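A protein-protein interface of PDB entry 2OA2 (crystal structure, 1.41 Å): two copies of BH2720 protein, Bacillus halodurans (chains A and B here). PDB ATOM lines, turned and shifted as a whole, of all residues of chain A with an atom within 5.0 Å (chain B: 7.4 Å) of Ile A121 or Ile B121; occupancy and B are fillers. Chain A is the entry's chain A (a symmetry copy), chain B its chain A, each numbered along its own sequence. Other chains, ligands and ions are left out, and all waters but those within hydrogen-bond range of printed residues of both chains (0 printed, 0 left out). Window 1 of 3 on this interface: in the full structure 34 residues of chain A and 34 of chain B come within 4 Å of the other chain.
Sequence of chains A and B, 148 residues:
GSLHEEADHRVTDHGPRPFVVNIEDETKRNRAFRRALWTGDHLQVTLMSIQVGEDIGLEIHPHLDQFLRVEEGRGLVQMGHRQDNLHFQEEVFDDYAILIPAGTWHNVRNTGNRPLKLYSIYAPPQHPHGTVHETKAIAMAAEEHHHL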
ATOM      1  N   LEU A  43     -23.845   9.026   5.067  1.00  0.00           N
ATOM      2  CA  LEU A  43     -22.827   8.003   5.007  1.00  0.00           C
ATOM      3  C   LEU A  43     -21.484   8.537   5.413  1.00  0.00           C
ATOM      4  O   LEU A  43     -21.222   9.733   5.396  1.00  0.00           O
ATOM      5  CB  LEU A  43     -22.791   7.322   3.652  1.00  0.00           C
ATOM      6  CG  LEU A  43     -22.186   8.042   2.470  1.00  0.00           C
ATOM      7  CD1 LEU A  43     -20.629   8.042   2.445  1.00  0.00           C
ATOM      8  CD2 LEU A  43     -22.751   7.490   1.128  1.00  0.00           C
ATOM      9  N   GLN A  44     -20.625   7.609   5.847  1.00  0.00           N
ATOM     10  CA  GLN A  44     -19.288   7.919   6.286  1.00  0.00           C
ATOM     11  C   GLN A  44     -18.273   6.957   5.720  1.00  0.00           C
ATOM     12  O   GLN A  44     -18.492   5.747   5.779  1.00  0.00           O
ATOM     13  CB  GLN A  44     -19.247   7.830   7.791  1.00  0.00           C
ATOM     14  CG  GLN A  44     -17.836   7.922   8.423  1.00  0.00           C
ATOM     15  CD  GLN A  44     -17.912   8.002   9.937  1.00  0.00           C
ATOM     16  OE1 GLN A  44     -18.404   7.051  10.583  1.00  0.00           O
ATOM     17  NE2 GLN A  44     -17.496   9.156  10.522  1.00  0.00           N
ATOM     18  N   VAL A  45     -17.170   7.484   5.191  1.00  0.00           N
ATOM     19  CA  VAL A  45     -16.075   6.685   4.642  1.00  0.00           C
ATOM     20  C   VAL A  45     -14.897   6.745   5.589  1.00  0.00           C
ATOM     21  O   VAL A  45     -14.456   7.849   5.957  1.00  0.00           O
ATOM     22  CB  VAL A  45     -15.641   7.226   3.251  1.00  0.00           C
ATOM     23  CG1 VAL A  45     -14.571   6.298   2.682  1.00  0.00           C
ATOM     24  CG2 VAL A  45     -16.821   7.413   2.305  1.00  0.00           C
ATOM     25  N   ASP A  65     -25.853  -0.317   8.101  1.00  0.00           N
ATOM     26  CA  ASP A  65     -25.224  -1.252   7.155  1.00  0.00           C
ATOM     27  C   ASP A  65     -23.786  -0.789   6.929  1.00  0.00           C
ATOM     28  O   ASP A  65     -23.468   0.392   7.037  1.00  0.00           O
ATOM     29  CB  ASP A  65     -25.932  -1.235   5.792  1.00  0.00           C
ATOM     30  CG  ASP A  65     -27.279  -1.911   5.785  1.00  0.00           C
ATOM     31  OD1 ASP A  65     -27.623  -2.660   6.763  1.00  0.00           O
ATOM     32  OD2 ASP A  65     -28.048  -1.669   4.827  1.00  0.00           O
ATOM     33  N   GLN A  66     -22.914  -1.724   6.585  1.00  0.00           N
ATOM     34  CA  GLN A  66     -21.513  -1.377   6.302  1.00  0.00           C
ATOM     35  C   GLN A  66     -21.088  -2.048   4.982  1.00  0.00           C
ATOM     36  O   GLN A  66     -21.449  -3.224   4.710  1.00  0.00           O
ATOM     37  CB  GLN A  66     -20.627  -1.792   7.503  1.00  0.00           C
ATOM     38  CG  GLN A  66     -19.134  -1.300   7.470  1.00  0.00           C
ATOM     39  CD  GLN A  66     -18.309  -1.643   8.706  1.00  0.00           C
ATOM     40  OE1 GLN A  66     -18.810  -2.199   9.641  1.00  0.00           O
ATOM     41  NE2 GLN A  66     -17.026  -1.269   8.686  1.00  0.00           N
ATOM     42  N   PHE A  67     -20.353  -1.319   4.188  1.00  0.00           N
ATOM     43  CA  PHE A  67     -19.699  -1.799   2.975  1.00  0.00           C
ATOM     44  C   PHE A  67     -18.203  -1.682   3.202  1.00  0.00           C
ATOM     45  O   PHE A  67     -17.742  -0.596   3.544  1.00  0.00           O
ATOM     46  CB  PHE A  67     -20.151  -0.958   1.788  1.00  0.00           C
ATOM     47  CG  PHE A  67     -19.394  -1.177   0.513  1.00  0.00           C
ATOM     48  CD1 PHE A  67     -18.204  -0.488   0.268  1.00  0.00           C
ATOM     49  CD2 PHE A  67     -19.880  -2.033  -0.456  1.00  0.00           C
ATOM     50  CE1 PHE A  67     -17.513  -0.664  -0.895  1.00  0.00           C
ATOM     51  CE2 PHE A  67     -19.181  -2.193  -1.679  1.00  0.00           C
ATOM     52  CZ  PHE A  67     -18.009  -1.502  -1.868  1.00  0.00           C
ATOM     53  N   LEU A  68     -17.446  -2.742   2.950  1.00  0.00           N
ATOM     54  CA  LEU A  68     -15.975  -2.668   3.035  1.00  0.00           C
ATOM     55  C   LEU A  68     -15.403  -3.075   1.697  1.00  0.00           C
ATOM     56  O   LEU A  68     -15.926  -3.988   1.055  1.00  0.00           O
ATOM     57  CB  LEU A  68     -15.388  -3.561   4.158  1.00  0.00           C
ATOM     58  CG  LEU A  68     -15.731  -3.087   5.580  1.00  0.00           C
ATOM     59  CD1 LEU A  68     -17.123  -3.614   5.969  1.00  0.00           C
ATOM     60  CD2 LEU A  68     -14.776  -3.462   6.596  1.00  0.00           C
ATOM     61  N   TYR A 119     -11.188   0.254   2.765  1.00  0.00           N
ATOM     62  CA  TYR A 119     -12.071   1.321   3.202  1.00  0.00           C
ATOM     63  C   TYR A 119     -13.421   0.796   3.573  1.00  0.00           C
ATOM     64  O   TYR A 119     -13.858  -0.249   3.080  1.00  0.00           O
ATOM     65  CB  TYR A 119     -12.178   2.449   2.180  1.00  0.00           C
ATOM     66  CG  TYR A 119     -12.725   2.170   0.773  1.00  0.00           C
ATOM     67  CD1 TYR A 119     -14.129   2.267   0.473  1.00  0.00           C
ATOM     68  CD2 TYR A 119     -11.879   1.883  -0.277  1.00  0.00           C
ATOM     69  CE1 TYR A 119     -14.549   2.065  -0.820  1.00  0.00           C
ATOM     70  CE2 TYR A 119     -12.315   1.696  -1.546  1.00  0.00           C
ATOM     71  CZ  TYR A 119     -13.691   1.780  -1.814  1.00  0.00           C
ATOM     72  OH  TYR A 119     -14.011   1.565  -3.145  1.00  0.00           O
ATOM     73  N   SER A 120     -14.062   1.540   4.480  1.00  0.00           N
ATOM     74  CA  SER A 120     -15.327   1.164   5.048  1.00  0.00           C
ATOM     75  C   SER A 120     -16.323   2.306   4.849  1.00  0.00           C
ATOM     76  O   SER A 120     -15.959   3.493   4.994  1.00  0.00           O
ATOM     77  CB  SER A 120     -15.133   0.822   6.518  1.00  0.00           C
ATOM     78  OG  SER A 120     -16.342   0.865   7.236  1.00  0.00           O
ATOM     79  N   ILE A 121     -17.543   1.965   4.478  1.00  0.00           N
ATOM     80  CA  ILE A 121     -18.633   2.938   4.347  1.00  0.00           C
ATOM     81  C   ILE A 121     -19.691   2.488   5.346  1.00  0.00           C
ATOM     82  O   ILE A 121     -20.197   1.349   5.257  1.00  0.00           O
ATOM     83  CB  ILE A 121     -19.188   3.013   2.941  1.00  0.00           C
ATOM     84  CG1 ILE A 121     -18.047   3.509   2.008  1.00  0.00           C
ATOM     85  CG2 ILE A 121     -20.425   3.862   2.920  1.00  0.00           C
ATOM     86  CD1 ILE A 121     -18.378   3.450   0.592  1.00  0.00           C
ATOM     87  N   TYR A 122     -19.996   3.360   6.294  1.00  0.00           N
ATOM     88  CA  TYR A 122     -21.071   3.150   7.256  1.00  0.00           C
ATOM     89  C   TYR A 122     -22.287   3.983   6.852  1.00  0.00           C
ATOM     90  O   TYR A 122     -22.135   5.150   6.469  1.00  0.00           O
ATOM     91  CB  TYR A 122     -20.680   3.651   8.617  1.00  0.00           C
ATOM     92  CG  TYR A 122     -19.534   2.972   9.304  1.00  0.00           C
ATOM     93  CD1 TYR A 122     -18.257   3.459   9.143  1.00  0.00           C
ATOM     94  CD2 TYR A 122     -19.729   1.929  10.149  1.00  0.00           C
ATOM     95  CE1 TYR A 122     -17.193   2.861   9.786  1.00  0.00           C
ATOM     96  CE2 TYR A 122     -18.663   1.363  10.867  1.00  0.00           C
ATOM     97  CZ  TYR A 122     -17.399   1.843  10.675  1.00  0.00           C
ATOM     98  OH  TYR A 122     -16.321   1.307  11.363  1.00  0.00           O
ATOM     99  N   ALA A 123     -23.489   3.406   6.920  1.00  0.00           N
ATOM    100  CA  ALA A 123     -24.734   4.162   6.668  1.00  0.00           C
ATOM    101  C   ALA A 123     -25.771   3.757   7.684  1.00  0.00           C
ATOM    102  O   ALA A 123     -26.162   2.590   7.720  1.00  0.00           O
ATOM    103  CB  ALA A 123     -25.266   3.851   5.301  1.00  0.00           C
ATOM    104  N   HIS B  42     -30.227  -0.002   4.956  1.00  0.00           N
ATOM    105  CA  HIS B  42     -29.566   1.305   5.171  1.00  0.00           C
ATOM    106  C   HIS B  42     -28.667   1.772   4.025  1.00  0.00           C
ATOM    107  O   HIS B  42     -28.516   2.985   3.846  1.00  0.00           O
ATOM    108  CB  HIS B  42     -28.798   1.336   6.494  1.00  0.00           C
ATOM    109  CG  HIS B  42     -29.631   0.918   7.644  1.00  0.00           C
ATOM    110  ND1 HIS B  42     -30.581   1.754   8.197  1.00  0.00           N
ATOM    111  CD2 HIS B  42     -29.669  -0.234   8.352  1.00  0.00           C
ATOM    112  CE1 HIS B  42     -31.169   1.110   9.200  1.00  0.00           C
ATOM    113  NE2 HIS B  42     -30.643  -0.095   9.310  1.00  0.00           N
ATOM    114  N   LEU B  43     -28.141   0.856   3.229  1.00  0.00           N
ATOM    115  CA  LEU B  43     -27.401   1.234   2.047  1.00  0.00           C
ATOM    116  C   LEU B  43     -27.691   0.313   0.897  1.00  0.00           C
ATOM    117  O   LEU B  43     -28.155  -0.808   1.057  1.00  0.00           O
ATOM    118  CB  LEU B  43     -25.916   1.358   2.327  1.00  0.00           C
ATOM    119  CG  LEU B  43     -25.081   0.109   2.491  1.00  0.00           C
ATOM    120  CD1 LEU B  43     -24.710  -0.598   1.155  1.00  0.00           C
ATOM    121  CD2 LEU B  43     -23.799   0.398   3.328  1.00  0.00           C
ATOM    122  N   GLN B  44     -27.457   0.841  -0.309  1.00  0.00           N
ATOM    123  CA  GLN B  44     -27.677   0.120  -1.538  1.00  0.00           C
ATOM    124  C   GLN B  44     -26.528   0.289  -2.501  1.00  0.00           C
ATOM    125  O   GLN B  44     -26.084   1.418  -2.718  1.00  0.00           O
ATOM    126  CB  GLN B  44     -28.929   0.654  -2.187  1.00  0.00           C
ATOM    127  CG  GLN B  44     -29.201   0.145  -3.624  1.00  0.00           C
ATOM    128  CD  GLN B  44     -30.563   0.592  -4.122  1.00  0.00           C
ATOM    129  OE1 GLN B  44     -30.805   1.813  -4.249  1.00  0.00           O
ATOM    130  NE2 GLN B  44     -31.494  -0.373  -4.343  1.00  0.00           N
ATOM    131  N   VAL B  45     -26.059  -0.814  -3.082  1.00  0.00           N
ATOM    132  CA  VAL B  45     -24.980  -0.812  -4.069  1.00  0.00           C
ATOM    133  C   VAL B  45     -25.562  -1.091  -5.438  1.00  0.00           C
ATOM    134  O   VAL B  45     -26.277  -2.094  -5.611  1.00  0.00           O
ATOM    135  CB  VAL B  45     -23.923  -1.901  -3.732  1.00  0.00           C
ATOM    136  CG1 VAL B  45     -22.774  -1.787  -4.730  1.00  0.00           C
ATOM    137  CG2 VAL B  45     -23.453  -1.827  -2.284  1.00  0.00           C
ATOM    138  N   THR B  46     -25.286  -0.233  -6.420  1.00  0.00           N
ATOM    139  CA  THR B  46     -25.668  -0.448  -7.798  1.00  0.00           C
ATOM    140  C   THR B  46     -24.390  -0.413  -8.653  1.00  0.00           C
ATOM    141  O   THR B  46     -23.385   0.195  -8.264  1.00  0.00           O
ATOM    142  CB  THR B  46     -26.661   0.599  -8.337  1.00  0.00           C
ATOM    143  OG1 THR B  46     -26.046   1.876  -8.396  1.00  0.00           O
ATOM    144  CG2 THR B  46     -27.864   0.661  -7.412  1.00  0.00           C
ATOM    145  N   LEU B  64     -30.420  11.731   0.782  1.00  0.00           N
ATOM    146  CA  LEU B  64     -29.406  10.691   0.784  1.00  0.00           C
ATOM    147  C   LEU B  64     -28.055  11.194   0.342  1.00  0.00           C
ATOM    148  O   LEU B  64     -27.981  12.148  -0.461  1.00  0.00           O
ATOM    149  CB  LEU B  64     -29.819   9.487  -0.040  1.00  0.00           C
ATOM    150  CG  LEU B  64     -30.104   9.656  -1.482  1.00  0.00           C
ATOM    151  CD1 LEU B  64     -28.827   9.665  -2.292  1.00  0.00           C
ATOM    152  CD2 LEU B  64     -31.062   8.544  -2.024  1.00  0.00           C
ATOM    153  N   ASP B  65     -27.019  10.524   0.821  1.00  0.00           N
ATOM    154  CA  ASP B  65     -25.640  10.723   0.349  1.00  0.00           C
ATOM    155  C   ASP B  65     -25.330   9.619  -0.660  1.00  0.00           C
ATOM    156  O   ASP B  65     -25.883   8.523  -0.602  1.00  0.00           O
ATOM    157  CB  ASP B  65     -24.628  10.594   1.496  1.00  0.00           C
ATOM    158  CG  ASP B  65     -24.620  11.761   2.450  1.00  0.00           C
ATOM    159  OD1 ASP B  65     -25.207  12.852   2.129  1.00  0.00           O
ATOM    160  OD2 ASP B  65     -24.072  11.600   3.564  1.00  0.00           O
ATOM    161  N   GLN B  66     -24.418   9.899  -1.577  1.00  0.00           N
ATOM    162  CA  GLN B  66     -24.014   8.890  -2.569  1.00  0.00           C
ATOM    163  C   GLN B  66     -22.476   8.841  -2.636  1.00  0.00           C
ATOM    164  O   GLN B  66     -21.794   9.899  -2.592  1.00  0.00           O
ATOM    165  CB  GLN B  66     -24.668   9.219  -3.934  1.00  0.00           C
ATOM    166  CG  GLN B  66     -24.526   8.127  -5.057  1.00  0.00           C
ATOM    167  CD  GLN B  66     -25.256   8.435  -6.360  1.00  0.00           C
ATOM    168  OE1 GLN B  66     -25.928   9.422  -6.466  1.00  0.00           O
ATOM    169  NE2 GLN B  66     -25.119   7.541  -7.342  1.00  0.00           N
ATOM    170  N   PHE B  67     -21.953   7.649  -2.732  1.00  0.00           N
ATOM    171  CA  PHE B  67     -20.541   7.372  -2.979  1.00  0.00           C
ATOM    172  C   PHE B  67     -20.454   6.675  -4.323  1.00  0.00           C
ATOM    173  O   PHE B  67     -21.134   5.669  -4.510  1.00  0.00           O
ATOM    174  CB  PHE B  67     -19.993   6.496  -1.859  1.00  0.00           C
ATOM    175  CG  PHE B  67     -18.622   5.935  -2.087  1.00  0.00           C
ATOM    176  CD1 PHE B  67     -18.453   4.747  -2.803  1.00  0.00           C
ATOM    177  CD2 PHE B  67     -17.509   6.560  -1.562  1.00  0.00           C
ATOM    178  CE1 PHE B  67     -17.213   4.215  -3.003  1.00  0.00           C
ATOM    179  CE2 PHE B  67     -16.222   5.992  -1.741  1.00  0.00           C
ATOM    180  CZ  PHE B  67     -16.107   4.828  -2.463  1.00  0.00           C
ATOM    181  N   LEU B  68     -19.591   7.140  -5.216  1.00  0.00           N
ATOM    182  CA  LEU B  68     -19.367   6.445  -6.498  1.00  0.00           C
ATOM    183  C   LEU B  68     -17.899   6.103  -6.602  1.00  0.00           C
ATOM    184  O   LEU B  68     -17.051   6.897  -6.190  1.00  0.00           O
ATOM    185  CB  LEU B  68     -19.806   7.284  -7.726  1.00  0.00           C
ATOM    186  CG  LEU B  68     -21.326   7.492  -7.832  1.00  0.00           C
ATOM    187  CD1 LEU B  68     -21.738   8.681  -6.946  1.00  0.00           C
ATOM    188  CD2 LEU B  68     -21.822   7.699  -9.172  1.00  0.00           C
ATOM    189  N   ARG B  69     -17.596   4.929  -7.131  1.00  0.00           N
ATOM    190  CA  ARG B  69     -16.227   4.576  -7.386  1.00  0.00           C
ATOM    191  C   ARG B  69     -16.095   4.173  -8.860  1.00  0.00           C
ATOM    192  O   ARG B  69     -16.809   3.279  -9.342  1.00  0.00           O
ATOM    193  CB  ARG B  69     -15.772   3.450  -6.443  1.00  0.00           C
ATOM    194  CG  ARG B  69     -14.252   3.408  -6.067  1.00  0.00           C
ATOM    195  CD  ARG B  69     -13.420   2.660  -7.040  1.00  0.00           C
ATOM    196  NE  ARG B  69     -12.119   2.230  -6.479  1.00  0.00           N
ATOM    197  CZ  ARG B  69     -11.084   1.837  -7.220  1.00  0.00           C
ATOM    198  NH1 ARG B  69     -11.164   1.857  -8.543  1.00  0.00           N
ATOM    199  NH2 ARG B  69      -9.950   1.429  -6.644  1.00  0.00           N
ATOM    200  N   ILE B  98     -16.125   9.503  -5.805  1.00  0.00           N
ATOM    201  CA  ILE B  98     -16.882  10.751  -5.816  1.00  0.00           C
ATOM    202  C   ILE B  98     -17.861  10.705  -4.650  1.00  0.00           C
ATOM    203  O   ILE B  98     -18.587   9.729  -4.522  1.00  0.00           O
ATOM    204  CB  ILE B  98     -17.719  10.891  -7.119  1.00  0.00           C
ATOM    205  CG1 ILE B  98     -16.858  10.644  -8.373  1.00  0.00           C
ATOM    206  CG2 ILE B  98     -18.477  12.192  -7.121  1.00  0.00           C
ATOM    207  CD1 ILE B  98     -17.637  10.357  -9.612  1.00  0.00           C
ATOM    208  N   LEU B  99     -17.845  11.732  -3.813  1.00  0.00           N
ATOM    209  CA  LEU B  99     -18.783  11.869  -2.705  1.00  0.00           C
ATOM    210  C   LEU B  99     -19.780  12.974  -3.052  1.00  0.00           C
ATOM    211  O   LEU B  99     -19.398  14.125  -3.399  1.00  0.00           O
ATOM    212  CB  LEU B  99     -18.080  12.166  -1.399  1.00  0.00           C
ATOM    213  CG  LEU B  99     -17.481  11.001  -0.641  1.00  0.00           C
ATOM    214  CD1 LEU B  99     -18.578  10.056  -0.222  1.00  0.00           C
ATOM    215  CD2 LEU B  99     -16.394  10.281  -1.449  1.00  0.00           C
ATOM    216  N   ILE B 100     -21.069  12.620  -2.986  1.00  0.00           N
ATOM    217  CA  ILE B 100     -22.166  13.510  -3.423  1.00  0.00           C
ATOM    218  C   ILE B 100     -23.085  13.684  -2.221  1.00  0.00           C
ATOM    219  O   ILE B 100     -23.927  12.818  -1.934  1.00  0.00           O
ATOM    220  CB  ILE B 100     -22.926  12.942  -4.608  1.00  0.00           C
ATOM    221  CG1 ILE B 100     -21.987  12.527  -5.752  1.00  0.00           C
ATOM    222  CG2 ILE B 100     -23.936  13.972  -5.065  1.00  0.00           C
ATOM    223  CD1 ILE B 100     -22.655  11.947  -6.981  1.00  0.00           C
ATOM    224  N   LEU B 118     -18.685   2.078 -13.161  1.00  0.00           N
ATOM    225  CA  LEU B 118     -18.601   2.499 -11.760  1.00  0.00           C
ATOM    226  C   LEU B 118     -19.605   1.735 -10.915  1.00  0.00           C
ATOM    227  O   LEU B 118     -20.540   1.116 -11.428  1.00  0.00           O
ATOM    228  CB  LEU B 118     -18.772   3.981 -11.608  1.00  0.00           C
ATOM    229  CG  LEU B 118     -20.068   4.547 -12.121  1.00  0.00           C
ATOM    230  CD1 LEU B 118     -21.118   4.451 -11.042  1.00  0.00           C
ATOM    231  CD2 LEU B 118     -19.928   6.052 -12.537  1.00  0.00           C
ATOM    232  N   TYR B 119     -19.373   1.769  -9.607  1.00  0.00           N
ATOM    233  CA  TYR B 119     -20.428   1.413  -8.674  1.00  0.00           C
ATOM    234  C   TYR B 119     -20.816   2.576  -7.817  1.00  0.00           C
ATOM    235  O   TYR B 119     -20.018   3.488  -7.579  1.00  0.00           O
ATOM    236  CB  TYR B 119     -20.075   0.195  -7.826  1.00  0.00           C
ATOM    237  CG  TYR B 119     -18.855   0.226  -6.895  1.00  0.00           C
ATOM    238  CD1 TYR B 119     -18.954   0.681  -5.532  1.00  0.00           C
ATOM    239  CD2 TYR B 119     -17.629  -0.247  -7.309  1.00  0.00           C
ATOM    240  CE1 TYR B 119     -17.839   0.628  -4.731  1.00  0.00           C
ATOM    241  CE2 TYR B 119     -16.545  -0.297  -6.497  1.00  0.00           C
ATOM    242  CZ  TYR B 119     -16.659   0.166  -5.176  1.00  0.00           C
ATOM    243  OH  TYR B 119     -15.483   0.066  -4.451  1.00  0.00           O
ATOM    244  N   SER B 120     -22.078   2.529  -7.380  1.00  0.00           N
ATOM    245  CA  SER B 120     -22.684   3.591  -6.625  1.00  0.00           C
ATOM    246  C   SER B 120     -23.248   3.022  -5.325  1.00  0.00           C
ATOM    247  O   SER B 120     -23.825   1.913  -5.319  1.00  0.00           O
ATOM    248  CB  SER B 120     -23.759   4.257  -7.473  1.00  0.00           C
ATOM    249  OG  SER B 120     -24.670   4.992  -6.694  1.00  0.00           O
ATOM    250  N   ILE B 121     -23.048   3.737  -4.233  1.00  0.00           N
ATOM    251  CA  ILE B 121     -23.615   3.372  -2.930  1.00  0.00           C
ATOM    252  C   ILE B 121     -24.515   4.540  -2.547  1.00  0.00           C
ATOM    253  O   ILE B 121     -24.039   5.691  -2.436  1.00  0.00           O
ATOM    254  CB  ILE B 121     -22.558   3.113  -1.880  1.00  0.00           C
ATOM    255  CG1 ILE B 121     -21.717   1.890  -2.346  1.00  0.00           C
ATOM    256  CG2 ILE B 121     -23.198   2.952  -0.532  1.00  0.00           C
ATOM    257  CD1 ILE B 121     -20.541   1.638  -1.528  1.00  0.00           C
ATOM    258  N   TYR B 122     -25.795   4.250  -2.375  1.00  0.00           N
ATOM    259  CA  TYR B 122     -26.774   5.212  -1.886  1.00  0.00           C
ATOM    260  C   TYR B 122     -27.070   4.935  -0.413  1.00  0.00           C
ATOM    261  O   TYR B 122     -27.230   3.770  -0.025  1.00  0.00           O
ATOM    262  CB  TYR B 122     -28.088   5.051  -2.594  1.00  0.00           C
ATOM    263  CG  TYR B 122     -28.120   5.321  -4.069  1.00  0.00           C
ATOM    264  CD1 TYR B 122     -27.914   4.290  -4.955  1.00  0.00           C
ATOM    265  CD2 TYR B 122     -28.427   6.548  -4.559  1.00  0.00           C
ATOM    266  CE1 TYR B 122     -27.963   4.515  -6.316  1.00  0.00           C
ATOM    267  CE2 TYR B 122     -28.554   6.770  -5.940  1.00  0.00           C
ATOM    268  CZ  TYR B 122     -28.321   5.740  -6.807  1.00  0.00           C
ATOM    269  OH  TYR B 122     -28.434   5.922  -8.176  1.00  0.00           O
ATOM    270  N   ALA B 123     -27.140   5.978   0.417  1.00  0.00           N
ATOM    271  CA  ALA B 123     -27.541   5.826   1.832  1.00  0.00           C
ATOM    272  C   ALA B 123     -28.470   6.953   2.205  1.00  0.00           C
ATOM    273  O   ALA B 123     -28.065   8.114   2.159  1.00  0.00           O
ATOM    274  CB  ALA B 123     -26.338   5.891   2.725  1.00  0.00           C
ATOM    275  N   PRO B 124     -29.712   6.652   2.586  1.00  0.00           N
ATOM    276  CA  PRO B 124     -30.384   5.368   2.497  1.00  0.00           C
ATOM    277  C   PRO B 124     -30.612   4.952   1.025  1.00  0.00           C
ATOM    278  O   PRO B 124     -30.267   5.673   0.087  1.00  0.00           O
ATOM    279  CB  PRO B 124     -31.732   5.599   3.197  1.00  0.00           C
ATOM    280  CG  PRO B 124     -31.600   6.932   3.876  1.00  0.00           C
ATOM    281  CD  PRO B 124     -30.545   7.703   3.209  1.00  0.00           C
ATOM    282  N   PRO B 125     -31.169   3.745   0.815  1.00  0.00           N
ATOM    283  CA  PRO B 125     -31.391   3.277  -0.560  1.00  0.00           C
ATOM    284  C   PRO B 125     -32.302   4.171  -1.399  1.00  0.00           C
ATOM    285  O   PRO B 125     -33.182   4.846  -0.843  1.00  0.00           O
ATOM    286  CB  PRO B 125     -32.016   1.901  -0.354  1.00  0.00           C
ATOM    287  CG  PRO B 125     -31.482   1.470   0.951  1.00  0.00           C
ATOM    288  CD  PRO B 125     -31.470   2.703   1.811  1.00  0.00           C
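Printed residues of chain A that touch a printed residue of chain B: Leu A43, Asp A65, Gln A66, Phe A67, Tyr A119, Ile A121 and Ala A123.
Hydrophobic or aromatic side chains of chain A that line the printed part of chain B: Leu A43, Phe A67, Tyr A119, Ile A121 and Ala A123.
Of the 22 printed residues of chain B, 10 touch a printed residue of chain A.
Printed residues of chain B that touch a printed residue of chain A: His B42, Leu B43, Asp B65, Gln B66, Phe B67, Arg B69, Leu B99, Tyr B119, Ile B121 and Ala B123.
Hydrophobic or aromatic side chains of chain B within 4 Å of the printed part of chain A: His B42, Leu B43, Phe B67, Leu B99, Tyr B119, Ile B121 and Ala B123.
Among the printed residues, 19 pairs touch across the chains.
Among the printed residues, no Asp or Glu carboxylate lies within 4 Å of a Lys or Arg side-chain nitrogen of the other chain.
Leu A43 touches Gln B66.
Leu B43 touches Gln A66 (CD2 to N, 3.99 Å).
N of Phe A67 touches CD2 of Leu B43, 3.9 Å away.
Phe A67 touches Ile B121.
CG of Arg B69 touches OH of Tyr A119, 3.5 Å away.
Ile A121 touches Phe B67.
Ile A121 touches Ile B121 (CD1 to CD1, 3.5 Å).
Ala A123 touches His B42 (O to CB, 3.2 Å).
CB of Ala A123 touches CB of Leu B43 (3.9 Å).
CB of Ala B123 touches CB of Ala A123, at 3.5 Å.
The side-chain carboxylate of Asp A65 lies within hydrogen-bond range of the backbone NH of His B42 (2.7 Å).
The backbone NH of Leu B43 lies within hydrogen-bond range of the side-chain carboxylate of Asp A65 (3.0 Å).
The side-chain carboxylate (OD2) of Asp B65 lies within hydrogen-bond range of the backbone NH (N) of Leu A43 (3.0 Å).
OH of Tyr B119 is in hydrogen-bond range of OH of Tyr A119 (2.5 Å).
Leu A43 touches Gln B66, and with the chains exchanged Gln A66 touches Leu B43.
Leu A43 touches Phe B67, and with the chains exchanged Phe A67 touches Leu B43.
Ile A121 touches its own counterpart, Ile B121.
Ala A123 touches its own counterpart, Ala B123.
Of the printed residues of chain B, Asp A65 touches His B42 and Leu B43.
Ser A120 touches none of the printed residues of chain B.
Printed residues of chain A within 4 Å of Leu B43: Asp A65, Gln A66, Phe A67 and Ala A123.
Val B45 touches none of the printed residues of chain A.
Of the printed residues of chain A, Arg B69 touches Tyr A119 (3.5 Å).
Of the printed residues of chain A, Leu B99 touches Leu A43.
Ile B121 touches just these residues of chain A: Phe A67 and Ile A121.
Of the printed residues of chain A, Ala B123 touches Leu A43 (3.9 Å) and Ala A123 (3.5 Å).
The nearest printed residue of chain A that does not touch Phe B67 is Val A45 (4.02 Å).
The backbone NH (N) of Asp B65 is in hydrogen-bond range of the backbone carbonyl oxygen (O) of Ala B123, 2.9 Å away.
O of Gln B66 lies within hydrogen-bond range of N of Ile B100, at 2.8 Å.
NE2 of Gln B66 is in hydrogen-bond range of OG of Ser B120 (2.7 Å).
The backbone NH (N) of Ile B121 sits at hydrogen-bond distance from the backbone carbonyl oxygen (O) of Phe B67 (2.7 Å).
The backbone carbonyl oxygen of Tyr B119 sits at hydrogen-bond distance from the backbone NH of Arg B69 (2.9 Å).
NE2 of Gln A66 sits at hydrogen-bond distance from OG of Ser A120 (2.7 Å).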
